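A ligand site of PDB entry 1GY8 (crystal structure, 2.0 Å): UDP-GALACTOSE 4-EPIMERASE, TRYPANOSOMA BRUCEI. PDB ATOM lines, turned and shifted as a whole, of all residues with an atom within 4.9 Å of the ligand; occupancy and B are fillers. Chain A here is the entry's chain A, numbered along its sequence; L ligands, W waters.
The side-chain amino group (NZ) of Lys 179 is in hydrogen-bond range of an oxygen (O12) of the ligand, 2.9 Å away. O9 of the ligand is in hydrogen-bond range of N of Ile 14, 2.8 Å away. OD1 of Asp 77 sits at hydrogen-bond distance from N3 of the ligand, 2.9 Å away. The backbone carbonyl oxygen (O) of Met 100 lies within hydrogen-bond range of an oxygen (O12) of the ligand (2.9 Å). The backbone NH (N) of Gly 38 is in hydrogen-bond range of an oxygen (O6) of the ligand, 2.8 Å away. The backbone NH (N) of Ala 205 is in hydrogen-bond range of an oxygen (O14) of the ligand, at 3.3 Å. The backbone NH (N) of Val 37 is in hydrogen-bond range of an oxygen (O6) of the ligand (3.1 Å). A nitrogen (N4) of the ligand sits at hydrogen-bond distance from the backbone NH (N) of Val 78 (3.1 Å). O2 of the ligand is in hydrogen-bond range of N of Tyr 13. The side-chain hydroxyl (OH) of Tyr 175 lies within hydrogen-bond range of an oxygen (O13) of the ligand. O5 of the ligand is in hydrogen-bond range of N of Gly 12, at 3.3 Å. An oxygen (O6) of the ligand is in hydrogen-bond range of the side-chain carboxylate of Asp 34, 2.6 Å away. N of Ser 35 sits at hydrogen-bond distance from N5 of the ligand (3.1 Å). The side-chain amide oxygen (OD1) of Asn 119 lies within hydrogen-bond range of a nitrogen (N3) of the ligand (2.8 Å). The side-chain hydroxyl (OG) of Ser 35 lies close to a nitrogen (N5) of the ligand (3.5 Å).
The guanidinium group (NH2) of Arg 79 lies close to the side-chain amide oxygen (OD1) of Asn 119 (3.4 Å). OG of Ser 142 lies within hydrogen-bond range of OH of Tyr 202 (2.6 Å). OD2 of Asp 77 lies within salt-bridge range of NH2 of Arg 79, 3.0 Å away. OD1 of Asp 34 is in hydrogen-bond range of N of Leu 36. The side-chain amino group (NZ) of Lys 179 lies within hydrogen-bond range of the backbone carbonyl oxygen (O) of Ser 142 (2.8 Å). N of Gly 76 lies within hydrogen-bond range of O of Asp 34, 3.0 Å away. The backbone carbonyl oxygen (O) of Ser 143 is in hydrogen-bond range of the backbone NH (N) of Tyr 202, at 3.3 Å. The backbone carbonyl oxygen (O) of Leu 36 lies close to the side-chain hydroxyl (OG1) of Thr 39 (3.3 Å).
Residues that only touch the ligand: Gly 9, Ala 11, Leu 36, Thr 39, Gly 76, Arg 79, Cys 101, Ala 102, Leu 104, Ser 142, Ser 143, Ser 144, Tyr 202, Phe 203 and His 223. Within 4 Å of the ligand: Gly 9, Ala 11, Gly 12, Tyr 13, Ile 14, Asp 34, Ser 35, Leu 36, Val 37, Gly 38, Thr 39, Gly 76, Asp 77, Val 78, Arg 79, Met 100, Cys 101, Ala 102, Leu 104, Asn 119, Ser 142, Ser 143, Ser 144, Tyr 175, Lys 179, Tyr 202, Phe 203, Ala 205 and His 223. The nearest printed residue that does not touch the ligand is Gly 15 (4.1 Å).
Water W6 bridges an oxygen (O2) of the ligand (2.7 Å) and the backbone carbonyl oxygen of Gly 38 (2.8 Å). Water W4 bridges the backbone carbonyl oxygen of Ala 205 and an oxygen (O14) of the ligand. Water W8 bridges N7 of the ligand (2.9 Å) and O of Ala 205 (3.4 Å). Water W2 bridges the backbone carbonyl oxygen (O) of Ala 102 (2.8 Å) and an oxygen (O1) of the ligand (2.9 Å). Water W3 bridges the side-chain hydroxyl of Tyr 175 and the side-chain hydroxyl of Ser 144. Water W11 lies within hydrogen-bond range of the side-chain hydroxyl (OG) of Ser 144, the backbone carbonyl oxygen (O) of Tyr 202 and the backbone carbonyl oxygen (O) of Phe 203.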
ATOM      1  N   GLY A   9      19.116 -20.674   9.467  1.00  0.00           N
ATOM      2  CA  GLY A   9      17.916 -20.915  10.259  1.00  0.00           C
ATOM      3  C   GLY A   9      18.204 -21.959  11.329  1.00  0.00           C
ATOM      4  O   GLY A   9      17.297 -22.559  11.895  1.00  0.00           O
ATOM      5  N   ALA A  11      19.085 -21.691  14.391  1.00  0.00           N
ATOM      6  CA  ALA A  11      18.680 -21.393  15.757  1.00  0.00           C
ATOM      7  C   ALA A  11      17.202 -21.713  15.992  1.00  0.00           C
ATOM      8  O   ALA A  11      16.698 -21.568  17.104  1.00  0.00           O
ATOM      9  CB  ALA A  11      18.945 -19.923  16.080  1.00  0.00           C
ATOM     10  N   GLY A  12      16.526 -22.156  14.941  1.00  0.00           N
ATOM     11  CA  GLY A  12      15.113 -22.486  15.049  1.00  0.00           C
ATOM     12  C   GLY A  12      14.800 -23.823  15.686  1.00  0.00           C
ATOM     13  O   GLY A  12      15.678 -24.533  16.179  1.00  0.00           O
ATOM     14  N   TYR A  13      13.512 -24.173  15.670  1.00  0.00           N
ATOM     15  CA  TYR A  13      13.020 -25.409  16.243  1.00  0.00           C
ATOM     16  C   TYR A  13      13.675 -26.649  15.636  1.00  0.00           C
ATOM     17  O   TYR A  13      14.334 -27.416  16.342  1.00  0.00           O
ATOM     18  CB  TYR A  13      11.506 -25.459  16.079  1.00  0.00           C
ATOM     19  CG  TYR A  13      10.834 -26.777  16.395  1.00  0.00           C
ATOM     20  CD1 TYR A  13      11.125 -27.470  17.571  1.00  0.00           C
ATOM     21  CD2 TYR A  13       9.850 -27.300  15.547  1.00  0.00           C
ATOM     22  CE1 TYR A  13      10.462 -28.667  17.887  1.00  0.00           C
ATOM     23  CE2 TYR A  13       9.178 -28.478  15.850  1.00  0.00           C
ATOM     24  CZ  TYR A  13       9.489 -29.152  17.014  1.00  0.00           C
ATOM     25  OH  TYR A  13       8.807 -30.311  17.313  1.00  0.00           O
ATOM     26  N   ILE A  14      13.496 -26.847  14.333  1.00  0.00           N
ATOM     27  CA  ILE A  14      14.072 -28.005  13.669  1.00  0.00           C
ATOM     28  C   ILE A  14      15.586 -27.848  13.552  1.00  0.00           C
ATOM     29  O   ILE A  14      16.331 -28.834  13.648  1.00  0.00           O
ATOM     30  CB  ILE A  14      13.446 -28.198  12.276  1.00  0.00           C
ATOM     31  CG1 ILE A  14      11.931 -28.362  12.414  1.00  0.00           C
ATOM     32  CG2 ILE A  14      14.043 -29.430  11.594  1.00  0.00           C
ATOM     33  CD1 ILE A  14      11.203 -28.555  11.089  1.00  0.00           C
ATOM     34  N   GLY A  15      16.044 -26.613  13.353  1.00  0.00           N
ATOM     35  CA  GLY A  15      17.468 -26.367  13.228  1.00  0.00           C
ATOM     36  C   GLY A  15      18.253 -26.743  14.475  1.00  0.00           C
ATOM     37  O   GLY A  15      19.333 -27.323  14.377  1.00  0.00           O
ATOM     38  N   VAL A  33      23.787 -19.524  10.838  1.00  0.00           N
ATOM     39  CA  VAL A  33      23.482 -18.164  10.416  1.00  0.00           C
ATOM     40  C   VAL A  33      21.972 -17.997  10.593  1.00  0.00           C
ATOM     41  O   VAL A  33      21.173 -18.636   9.903  1.00  0.00           O
ATOM     42  CB  VAL A  33      23.936 -17.880   8.950  1.00  0.00           C
ATOM     43  CG1 VAL A  33      23.450 -18.972   8.020  1.00  0.00           C
ATOM     44  CG2 VAL A  33      23.402 -16.527   8.490  1.00  0.00           C
ATOM     45  N   ASP A  34      21.579 -17.149  11.537  1.00  0.00           N
ATOM     46  CA  ASP A  34      20.174 -16.949  11.854  1.00  0.00           C
ATOM     47  C   ASP A  34      19.955 -15.496  12.273  1.00  0.00           C
ATOM     48  O   ASP A  34      20.805 -14.909  12.953  1.00  0.00           O
ATOM     49  CB  ASP A  34      19.797 -17.902  12.995  1.00  0.00           C
ATOM     50  CG  ASP A  34      18.314 -18.140  13.115  1.00  0.00           C
ATOM     51  OD1 ASP A  34      17.563 -17.191  13.421  1.00  0.00           O
ATOM     52  OD2 ASP A  34      17.891 -19.286  12.917  1.00  0.00           O
ATOM     53  N   SER A  35      18.835 -14.916  11.862  1.00  0.00           N
ATOM     54  CA  SER A  35      18.511 -13.520  12.174  1.00  0.00           C
ATOM     55  C   SER A  35      17.838 -13.425  13.540  1.00  0.00           C
ATOM     56  O   SER A  35      17.687 -12.335  14.090  1.00  0.00           O
ATOM     57  CB  SER A  35      17.587 -12.932  11.111  1.00  0.00           C
ATOM     58  OG  SER A  35      16.342 -13.615  11.099  1.00  0.00           O
ATOM     59  N   LEU A  36      17.427 -14.578  14.063  1.00  0.00           N
ATOM     60  CA  LEU A  36      16.748 -14.678  15.349  1.00  0.00           C
ATOM     61  C   LEU A  36      15.344 -14.093  15.291  1.00  0.00           C
ATOM     62  O   LEU A  36      14.741 -13.808  16.326  1.00  0.00           O
ATOM     63  CB  LEU A  36      17.560 -13.983  16.456  1.00  0.00           C
ATOM     64  CG  LEU A  36      19.018 -14.475  16.653  1.00  0.00           C
ATOM     65  CD1 LEU A  36      19.594 -13.846  17.924  1.00  0.00           C
ATOM     66  CD2 LEU A  36      19.046 -15.996  16.765  1.00  0.00           C
ATOM     67  N   VAL A  37      14.808 -13.922  14.087  1.00  0.00           N
ATOM     68  CA  VAL A  37      13.469 -13.385  13.918  1.00  0.00           C
ATOM     69  C   VAL A  37      12.430 -14.408  14.374  1.00  0.00           C
ATOM     70  O   VAL A  37      11.321 -14.053  14.770  1.00  0.00           O
ATOM     71  CB  VAL A  37      13.203 -13.005  12.428  1.00  0.00           C
ATOM     72  CG1 VAL A  37      13.207 -14.249  11.552  1.00  0.00           C
ATOM     73  CG2 VAL A  37      11.871 -12.268  12.308  1.00  0.00           C
ATOM     74  N   GLY A  38      12.812 -15.687  14.350  1.00  0.00           N
ATOM     75  CA  GLY A  38      11.893 -16.725  14.773  1.00  0.00           C
ATOM     76  C   GLY A  38      12.204 -17.240  16.175  1.00  0.00           C
ATOM     77  O   GLY A  38      11.625 -18.234  16.614  1.00  0.00           O
ATOM     78  N   THR A  39      13.112 -16.569  16.874  1.00  0.00           N
ATOM     79  CA  THR A  39      13.474 -16.991  18.222  1.00  0.00           C
ATOM     80  C   THR A  39      13.366 -15.840  19.220  1.00  0.00           C
ATOM     81  O   THR A  39      14.068 -15.809  20.226  1.00  0.00           O
ATOM     82  CB  THR A  39      14.919 -17.551  18.248  1.00  0.00           C
ATOM     83  OG1 THR A  39      15.853 -16.517  17.927  1.00  0.00           O
ATOM     84  CG2 THR A  39      15.058 -18.677  17.217  1.00  0.00           C
ATOM     85  N   GLY A  76      22.346 -12.627  11.687  1.00  0.00           N
ATOM     86  CA  GLY A  76      22.050 -11.739  10.591  1.00  0.00           C
ATOM     87  C   GLY A  76      21.093 -12.367   9.589  1.00  0.00           C
ATOM     88  O   GLY A  76      20.800 -13.560   9.667  1.00  0.00           O
ATOM     89  N   ASP A  77      20.622 -11.557   8.641  1.00  0.00           N
ATOM     90  CA  ASP A  77      19.694 -12.016   7.623  1.00  0.00           C
ATOM     91  C   ASP A  77      20.437 -12.537   6.378  1.00  0.00           C
ATOM     92  O   ASP A  77      21.351 -11.874   5.883  1.00  0.00           O
ATOM     93  CB  ASP A  77      18.779 -10.845   7.228  1.00  0.00           C
ATOM     94  CG  ASP A  77      17.497 -11.307   6.571  1.00  0.00           C
ATOM     95  OD1 ASP A  77      17.552 -12.036   5.555  1.00  0.00           O
ATOM     96  OD2 ASP A  77      16.414 -10.937   7.067  1.00  0.00           O
ATOM     97  N   VAL A  78      20.046 -13.712   5.871  1.00  0.00           N
ATOM     98  CA  VAL A  78      20.706 -14.292   4.702  1.00  0.00           C
ATOM     99  C   VAL A  78      20.478 -13.483   3.429  1.00  0.00           C
ATOM    100  O   VAL A  78      21.139 -13.674   2.412  1.00  0.00           O
ATOM    101  CB  VAL A  78      20.278 -15.770   4.455  1.00  0.00           C
ATOM    102  CG1 VAL A  78      20.711 -16.636   5.624  1.00  0.00           C
ATOM    103  CG2 VAL A  78      18.765 -15.858   4.247  1.00  0.00           C
ATOM    104  N   ARG A  79      19.517 -12.563   3.498  1.00  0.00           N
ATOM    105  CA  ARG A  79      19.233 -11.701   2.366  1.00  0.00           C
ATOM    106  C   ARG A  79      20.184 -10.506   2.355  1.00  0.00           C
ATOM    107  O   ARG A  79      20.215  -9.748   1.394  1.00  0.00           O
ATOM    108  CB  ARG A  79      17.786 -11.221   2.414  1.00  0.00           C
ATOM    109  CG  ARG A  79      16.776 -12.322   2.124  1.00  0.00           C
ATOM    110  CD  ARG A  79      15.352 -11.853   2.357  1.00  0.00           C
ATOM    111  NE  ARG A  79      15.135 -11.527   3.766  1.00  0.00           N
ATOM    112  CZ  ARG A  79      13.971 -11.135   4.276  1.00  0.00           C
ATOM    113  NH1 ARG A  79      12.909 -10.999   3.492  1.00  0.00           N
ATOM    114  NH2 ARG A  79      13.859 -10.896   5.581  1.00  0.00           N
ATOM    115  N   MET A 100      17.528 -23.821   6.146  1.00  0.00           N
ATOM    116  CA  MET A 100      16.328 -24.009   6.949  1.00  0.00           C
ATOM    117  C   MET A 100      15.554 -22.732   7.283  1.00  0.00           C
ATOM    118  O   MET A 100      14.491 -22.792   7.878  1.00  0.00           O
ATOM    119  CB  MET A 100      16.704 -24.722   8.254  1.00  0.00           C
ATOM    120  CG  MET A 100      17.622 -25.916   8.055  1.00  0.00           C
ATOM    121  SD  MET A 100      17.991 -26.783   9.596  1.00  0.00           S
ATOM    122  CE  MET A 100      16.575 -27.833   9.697  1.00  0.00           C
ATOM    123  N   CYS A 101      16.088 -21.573   6.926  1.00  0.00           N
ATOM    124  CA  CYS A 101      15.395 -20.318   7.246  1.00  0.00           C
ATOM    125  C   CYS A 101      14.186 -20.037   6.363  1.00  0.00           C
ATOM    126  O   CYS A 101      14.204 -20.271   5.144  1.00  0.00           O
ATOM    127  CB  CYS A 101      16.370 -19.157   7.150  1.00  0.00           C
ATOM    128  SG  CYS A 101      17.250 -19.158   5.604  1.00  0.00           S
ATOM    129  N   ALA A 102      13.127 -19.516   6.977  1.00  0.00           N
ATOM    130  CA  ALA A 102      11.900 -19.186   6.268  1.00  0.00           C
ATOM    131  C   ALA A 102      10.809 -18.750   7.239  1.00  0.00           C
ATOM    132  O   ALA A 102      10.993 -18.809   8.452  1.00  0.00           O
ATOM    133  CB  ALA A 102      11.419 -20.402   5.510  1.00  0.00           C
ATOM    134  N   PHE A 103       9.705 -18.274   6.684  1.00  0.00           N
ATOM    135  CA  PHE A 103       8.521 -17.939   7.465  1.00  0.00           C
ATOM    136  C   PHE A 103       7.655 -19.133   7.104  1.00  0.00           C
ATOM    137  O   PHE A 103       7.652 -19.559   5.956  1.00  0.00           O
ATOM    138  CB  PHE A 103       7.887 -16.616   7.006  1.00  0.00           C
ATOM    139  CG  PHE A 103       8.652 -15.403   7.430  1.00  0.00           C
ATOM    140  CD1 PHE A 103       9.192 -15.329   8.707  1.00  0.00           C
ATOM    141  CD2 PHE A 103       8.826 -14.335   6.568  1.00  0.00           C
ATOM    142  CE1 PHE A 103       9.918 -14.210   9.115  1.00  0.00           C
ATOM    143  CE2 PHE A 103       9.542 -13.207   6.964  1.00  0.00           C
ATOM    144  CZ  PHE A 103      10.093 -13.145   8.232  1.00  0.00           C
ATOM    145  N   LEU A 104       6.941 -19.698   8.078  1.00  0.00           N
ATOM    146  CA  LEU A 104       6.181 -20.908   7.805  1.00  0.00           C
ATOM    147  C   LEU A 104       4.761 -21.039   8.337  1.00  0.00           C
ATOM    148  O   LEU A 104       4.300 -22.163   8.599  1.00  0.00           O
ATOM    149  CB  LEU A 104       7.003 -22.114   8.293  1.00  0.00           C
ATOM    150  CG  LEU A 104       7.427 -22.070   9.772  1.00  0.00           C
ATOM    151  CD1 LEU A 104       7.568 -23.491  10.319  1.00  0.00           C
ATOM    152  CD2 LEU A 104       8.726 -21.295   9.913  1.00  0.00           C
ATOM    153  N   ASN A 119      10.961 -13.336   1.821  1.00  0.00           N
ATOM    154  CA  ASN A 119      11.856 -14.110   2.670  1.00  0.00           C
ATOM    155  C   ASN A 119      12.188 -15.497   2.154  1.00  0.00           C
ATOM    156  O   ASN A 119      13.354 -15.890   2.091  1.00  0.00           O
ATOM    157  CB  ASN A 119      11.292 -14.208   4.092  1.00  0.00           C
ATOM    158  CG  ASN A 119      12.338 -14.694   5.092  1.00  0.00           C
ATOM    159  OD1 ASN A 119      13.487 -14.273   5.051  1.00  0.00           O
ATOM    160  ND2 ASN A 119      11.931 -15.573   5.997  1.00  0.00           N
ATOM    161  N   SER A 142      15.189 -27.295   3.192  1.00  0.00           N
ATOM    162  CA  SER A 142      14.011 -27.627   3.979  1.00  0.00           C
ATOM    163  C   SER A 142      12.748 -27.342   3.184  1.00  0.00           C
ATOM    164  O   SER A 142      12.300 -26.196   3.135  1.00  0.00           O
ATOM    165  CB  SER A 142      13.944 -26.785   5.260  1.00  0.00           C
ATOM    166  OG  SER A 142      15.065 -26.973   6.095  1.00  0.00           O
ATOM    167  N   SER A 143      12.190 -28.373   2.566  1.00  0.00           N
ATOM    168  CA  SER A 143      10.957 -28.185   1.798  1.00  0.00           C
ATOM    169  C   SER A 143       9.776 -28.607   2.659  1.00  0.00           C
ATOM    170  O   SER A 143       9.933 -28.862   3.851  1.00  0.00           O
ATOM    171  CB  SER A 143      10.993 -29.009   0.502  1.00  0.00           C
ATOM    172  OG  SER A 143       9.942 -28.592  -0.357  1.00  0.00           O
ATOM    173  N   SER A 144       8.589 -28.695   2.059  1.00  0.00           N
ATOM    174  CA  SER A 144       7.402 -29.033   2.815  1.00  0.00           C
ATOM    175  C   SER A 144       6.337 -29.798   2.033  1.00  0.00           C
ATOM    176  O   SER A 144       6.294 -29.762   0.800  1.00  0.00           O
ATOM    177  CB  SER A 144       6.769 -27.750   3.376  1.00  0.00           C
ATOM    178  OG  SER A 144       5.489 -27.990   3.921  1.00  0.00           O
ATOM    179  N   TYR A 175       2.797 -20.045   0.885  1.00  0.00           N
ATOM    180  CA  TYR A 175       3.907 -20.713   1.572  1.00  0.00           C
ATOM    181  C   TYR A 175       4.330 -21.920   0.728  1.00  0.00           C
ATOM    182  O   TYR A 175       5.522 -22.110   0.471  1.00  0.00           O
ATOM    183  CB  TYR A 175       3.458 -21.181   2.957  1.00  0.00           C
ATOM    184  CG  TYR A 175       4.451 -22.126   3.623  1.00  0.00           C
ATOM    185  CD1 TYR A 175       5.690 -21.653   4.094  1.00  0.00           C
ATOM    186  CD2 TYR A 175       4.166 -23.481   3.767  1.00  0.00           C
ATOM    187  CE1 TYR A 175       6.594 -22.514   4.713  1.00  0.00           C
ATOM    188  CE2 TYR A 175       5.060 -24.342   4.386  1.00  0.00           C
ATOM    189  CZ  TYR A 175       6.269 -23.860   4.854  1.00  0.00           C
ATOM    190  OH  TYR A 175       7.132 -24.716   5.501  1.00  0.00           O
ATOM    191  N   LYS A 179       8.003 -22.644  -1.453  1.00  0.00           N
ATOM    192  CA  LYS A 179       8.846 -23.827  -1.261  1.00  0.00           C
ATOM    193  C   LYS A 179       9.043 -24.527  -2.601  1.00  0.00           C
ATOM    194  O   LYS A 179      10.130 -25.026  -2.894  1.00  0.00           O
ATOM    195  CB  LYS A 179       8.225 -24.803  -0.259  1.00  0.00           C
ATOM    196  CG  LYS A 179       8.306 -24.358   1.193  1.00  0.00           C
ATOM    197  CD  LYS A 179       9.759 -24.186   1.619  1.00  0.00           C
ATOM    198  CE  LYS A 179       9.880 -23.859   3.092  1.00  0.00           C
ATOM    199  NZ  LYS A 179      11.294 -23.601   3.482  1.00  0.00           N
ATOM    200  N   TYR A 202       9.608 -32.063   4.673  1.00  0.00           N
ATOM    201  CA  TYR A 202       9.191 -32.544   5.980  1.00  0.00           C
ATOM    202  C   TYR A 202       7.690 -32.440   5.954  1.00  0.00           C
ATOM    203  O   TYR A 202       7.119 -31.590   5.259  1.00  0.00           O
ATOM    204  CB  TYR A 202       9.649 -31.665   7.165  1.00  0.00           C
ATOM    205  CG  TYR A 202      11.027 -31.056   7.092  1.00  0.00           C
ATOM    206  CD1 TYR A 202      12.086 -31.734   6.513  1.00  0.00           C
ATOM    207  CD2 TYR A 202      11.265 -29.800   7.662  1.00  0.00           C
ATOM    208  CE1 TYR A 202      13.363 -31.177   6.495  1.00  0.00           C
ATOM    209  CE2 TYR A 202      12.542 -29.232   7.652  1.00  0.00           C
ATOM    210  CZ  TYR A 202      13.591 -29.931   7.066  1.00  0.00           C
ATOM    211  OH  TYR A 202      14.858 -29.384   7.049  1.00  0.00           O
ATOM    212  N   PHE A 203       7.038 -33.314   6.706  1.00  0.00           N
ATOM    213  CA  PHE A 203       5.602 -33.240   6.810  1.00  0.00           C
ATOM    214  C   PHE A 203       5.326 -32.485   8.117  1.00  0.00           C
ATOM    215  O   PHE A 203       5.831 -31.366   8.273  1.00  0.00           O
ATOM    216  CB  PHE A 203       4.997 -34.634   6.714  1.00  0.00           C
ATOM    217  CG  PHE A 203       4.806 -35.086   5.279  1.00  0.00           C
ATOM    218  CD1 PHE A 203       5.890 -35.072   4.397  1.00  0.00           C
ATOM    219  CD2 PHE A 203       3.547 -35.391   4.781  1.00  0.00           C
ATOM    220  CE1 PHE A 203       5.715 -35.349   3.046  1.00  0.00           C
ATOM    221  CE2 PHE A 203       3.351 -35.678   3.430  1.00  0.00           C
ATOM    222  CZ  PHE A 203       4.445 -35.643   2.556  1.00  0.00           C
ATOM    223  N   ASN A 204       4.593 -33.023   9.076  1.00  0.00           N
ATOM    224  CA  ASN A 204       4.380 -32.214  10.276  1.00  0.00           C
ATOM    225  C   ASN A 204       5.359 -32.468  11.399  1.00  0.00           C
ATOM    226  O   ASN A 204       5.187 -33.395  12.189  1.00  0.00           O
ATOM    227  CB  ASN A 204       2.930 -32.340  10.776  1.00  0.00           C
ATOM    228  CG  ASN A 204       1.947 -31.583   9.886  1.00  0.00           C
ATOM    229  OD1 ASN A 204       1.825 -31.873   8.701  1.00  0.00           O
ATOM    230  ND2 ASN A 204       1.277 -30.601  10.463  1.00  0.00           N
ATOM    231  N   ALA A 205       6.391 -31.636  11.460  1.00  0.00           N
ATOM    232  CA  ALA A 205       7.423 -31.744  12.481  1.00  0.00           C
ATOM    233  C   ALA A 205       6.848 -31.572  13.880  1.00  0.00           C
ATOM    234  O   ALA A 205       6.060 -30.664  14.129  1.00  0.00           O
ATOM    235  CB  ALA A 205       8.505 -30.708  12.227  1.00  0.00           C
ATOM    236  N   HIS A 223       1.413 -23.690  15.315  1.00  0.00           N
ATOM    237  CA  HIS A 223       1.213 -25.122  15.100  1.00  0.00           C
ATOM    238  C   HIS A 223       0.319 -25.824  16.108  1.00  0.00           C
ATOM    239  O   HIS A 223       0.321 -25.483  17.290  1.00  0.00           O
ATOM    240  CB  HIS A 223       2.563 -25.833  15.003  1.00  0.00           C
ATOM    241  CG  HIS A 223       3.357 -25.448  13.788  1.00  0.00           C
ATOM    242  ND1 HIS A 223       4.379 -24.529  13.824  1.00  0.00           N
ATOM    243  CD2 HIS A 223       3.210 -25.797  12.490  1.00  0.00           C
ATOM    244  CE1 HIS A 223       4.835 -24.327  12.604  1.00  0.00           C
ATOM    245  NE2 HIS A 223       4.143 -25.091  11.765  1.00  0.00           N
HETATM  246  P1  LIG L   1      11.666 -21.828  12.943  1.00  0.00           P
HETATM  247  O1  LIG L   1      11.035 -20.506  12.666  1.00  0.00           O
HETATM  248  O2  LIG L   1      11.806 -22.232  14.340  1.00  0.00           O
HETATM  249  O3  LIG L   1      13.115 -21.878  12.228  1.00  0.00           O
HETATM  250  C1  LIG L   1      13.457 -20.959  11.193  1.00  0.00           C
HETATM  251  C2  LIG L   1      14.675 -20.178  11.624  1.00  0.00           C
HETATM  252  O4  LIG L   1      15.062 -19.406  10.492  1.00  0.00           O
HETATM  253  C3  LIG L   1      14.323 -19.199  12.751  1.00  0.00           C
HETATM  254  O5  LIG L   1      15.326 -19.349  13.767  1.00  0.00           O
HETATM  255  C4  LIG L   1      14.408 -17.828  12.079  1.00  0.00           C
HETATM  256  O6  LIG L   1      14.975 -16.869  13.003  1.00  0.00           O
HETATM  257  C5  LIG L   1      15.327 -18.058  10.876  1.00  0.00           C
HETATM  258  N1  LIG L   1      15.153 -17.156   9.742  1.00  0.00           N
HETATM  259  C6  LIG L   1      14.016 -16.834   9.047  1.00  0.00           C
HETATM  260  N2  LIG L   1      14.307 -15.971   8.040  1.00  0.00           N
HETATM  261  C7  LIG L   1      15.623 -15.771   8.131  1.00  0.00           C
HETATM  262  C8  LIG L   1      16.428 -14.975   7.337  1.00  0.00           C
HETATM  263  N3  LIG L   1      15.941 -14.288   6.316  1.00  0.00           N
HETATM  264  N4  LIG L   1      17.798 -14.919   7.605  1.00  0.00           N
HETATM  265  C9  LIG L   1      18.314 -15.623   8.640  1.00  0.00           C
HETATM  266  N5  LIG L   1      17.531 -16.393   9.411  1.00  0.00           N
HETATM  267  C10 LIG L   1      16.169 -16.484   9.179  1.00  0.00           C
HETATM  268  O7  LIG L   1      10.896 -22.970  12.142  1.00  0.00           O
HETATM  269  P2  LIG L   1      11.086 -24.537  11.963  1.00  0.00           P
HETATM  270  O8  LIG L   1       9.844 -25.210  12.396  1.00  0.00           O
HETATM  271  O9  LIG L   1      12.332 -24.916  12.681  1.00  0.00           O
HETATM  272  O10 LIG L   1      11.278 -24.717  10.388  1.00  0.00           O
HETATM  273  C11 LIG L   1      12.572 -24.710   9.780  1.00  0.00           C
HETATM  274  C12 LIG L   1      12.432 -24.969   8.285  1.00  0.00           C
HETATM  275  O11 LIG L   1      11.680 -26.161   8.061  1.00  0.00           O
HETATM  276  C13 LIG L   1      11.700 -23.834   7.538  1.00  0.00           C
HETATM  277  O12 LIG L   1      12.280 -23.669   6.217  1.00  0.00           O
HETATM  278  C14 LIG L   1      10.249 -24.385   7.406  1.00  0.00           C
HETATM  279  O13 LIG L   1       9.576 -23.785   6.291  1.00  0.00           O
HETATM  280  C15 LIG L   1      10.530 -25.866   7.198  1.00  0.00           C
HETATM  281  N6  LIG L   1       9.395 -26.754   7.487  1.00  0.00           N
HETATM  282  C16 LIG L   1       8.854 -26.766   8.815  1.00  0.00           C
HETATM  283  C17 LIG L   1       7.789 -27.635   9.094  1.00  0.00           C
HETATM  284  C18 LIG L   1       7.155 -27.703  10.518  1.00  0.00           C
HETATM  285  O14 LIG L   1       6.233 -28.474  10.716  1.00  0.00           O
HETATM  286  N7  LIG L   1       7.694 -26.889  11.423  1.00  0.00           N
HETATM  287  C19 LIG L   1       7.266 -28.480   8.062  1.00  0.00           C
HETATM  288  C20 LIG L   1       7.807 -28.469   6.724  1.00  0.00           C
HETATM  289  C21 LIG L   1       8.881 -27.598   6.456  1.00  0.00           C
HETATM  290  O   HOH W   1       9.409 -22.536  15.834  1.00  0.00           O
HETATM  291  O   HOH W   2      11.153 -18.025  11.140  1.00  0.00           O
HETATM  292  O   HOH W   3       5.249 -26.314   6.937  1.00  0.00           O
HETATM  293  O   HOH W   4       4.608 -28.786  12.971  1.00  0.00           O
HETATM  294  O   HOH W   5      14.340 -23.046   4.315  1.00  0.00           O
HETATM  295  O   HOH W   6      12.075 -21.021  16.722  1.00  0.00           O
HETATM  296  O   HOH W   7       7.970 -24.276  14.088  1.00  0.00           O
HETATM  297  O   HOH W   8       6.526 -27.346  14.034  1.00  0.00           O
HETATM  298  O   HOH W   9      15.123 -24.240  12.310  1.00  0.00           O
HETATM  299  O   HOH W  10       4.102 -28.478   9.385  1.00  0.00           O
HETATM  300  O   HOH W  11       4.789 -29.719   5.851  1.00  0.00           O
HETATM  301  O   HOH W  12       8.520 -19.811  13.378  1.00  0.00           O
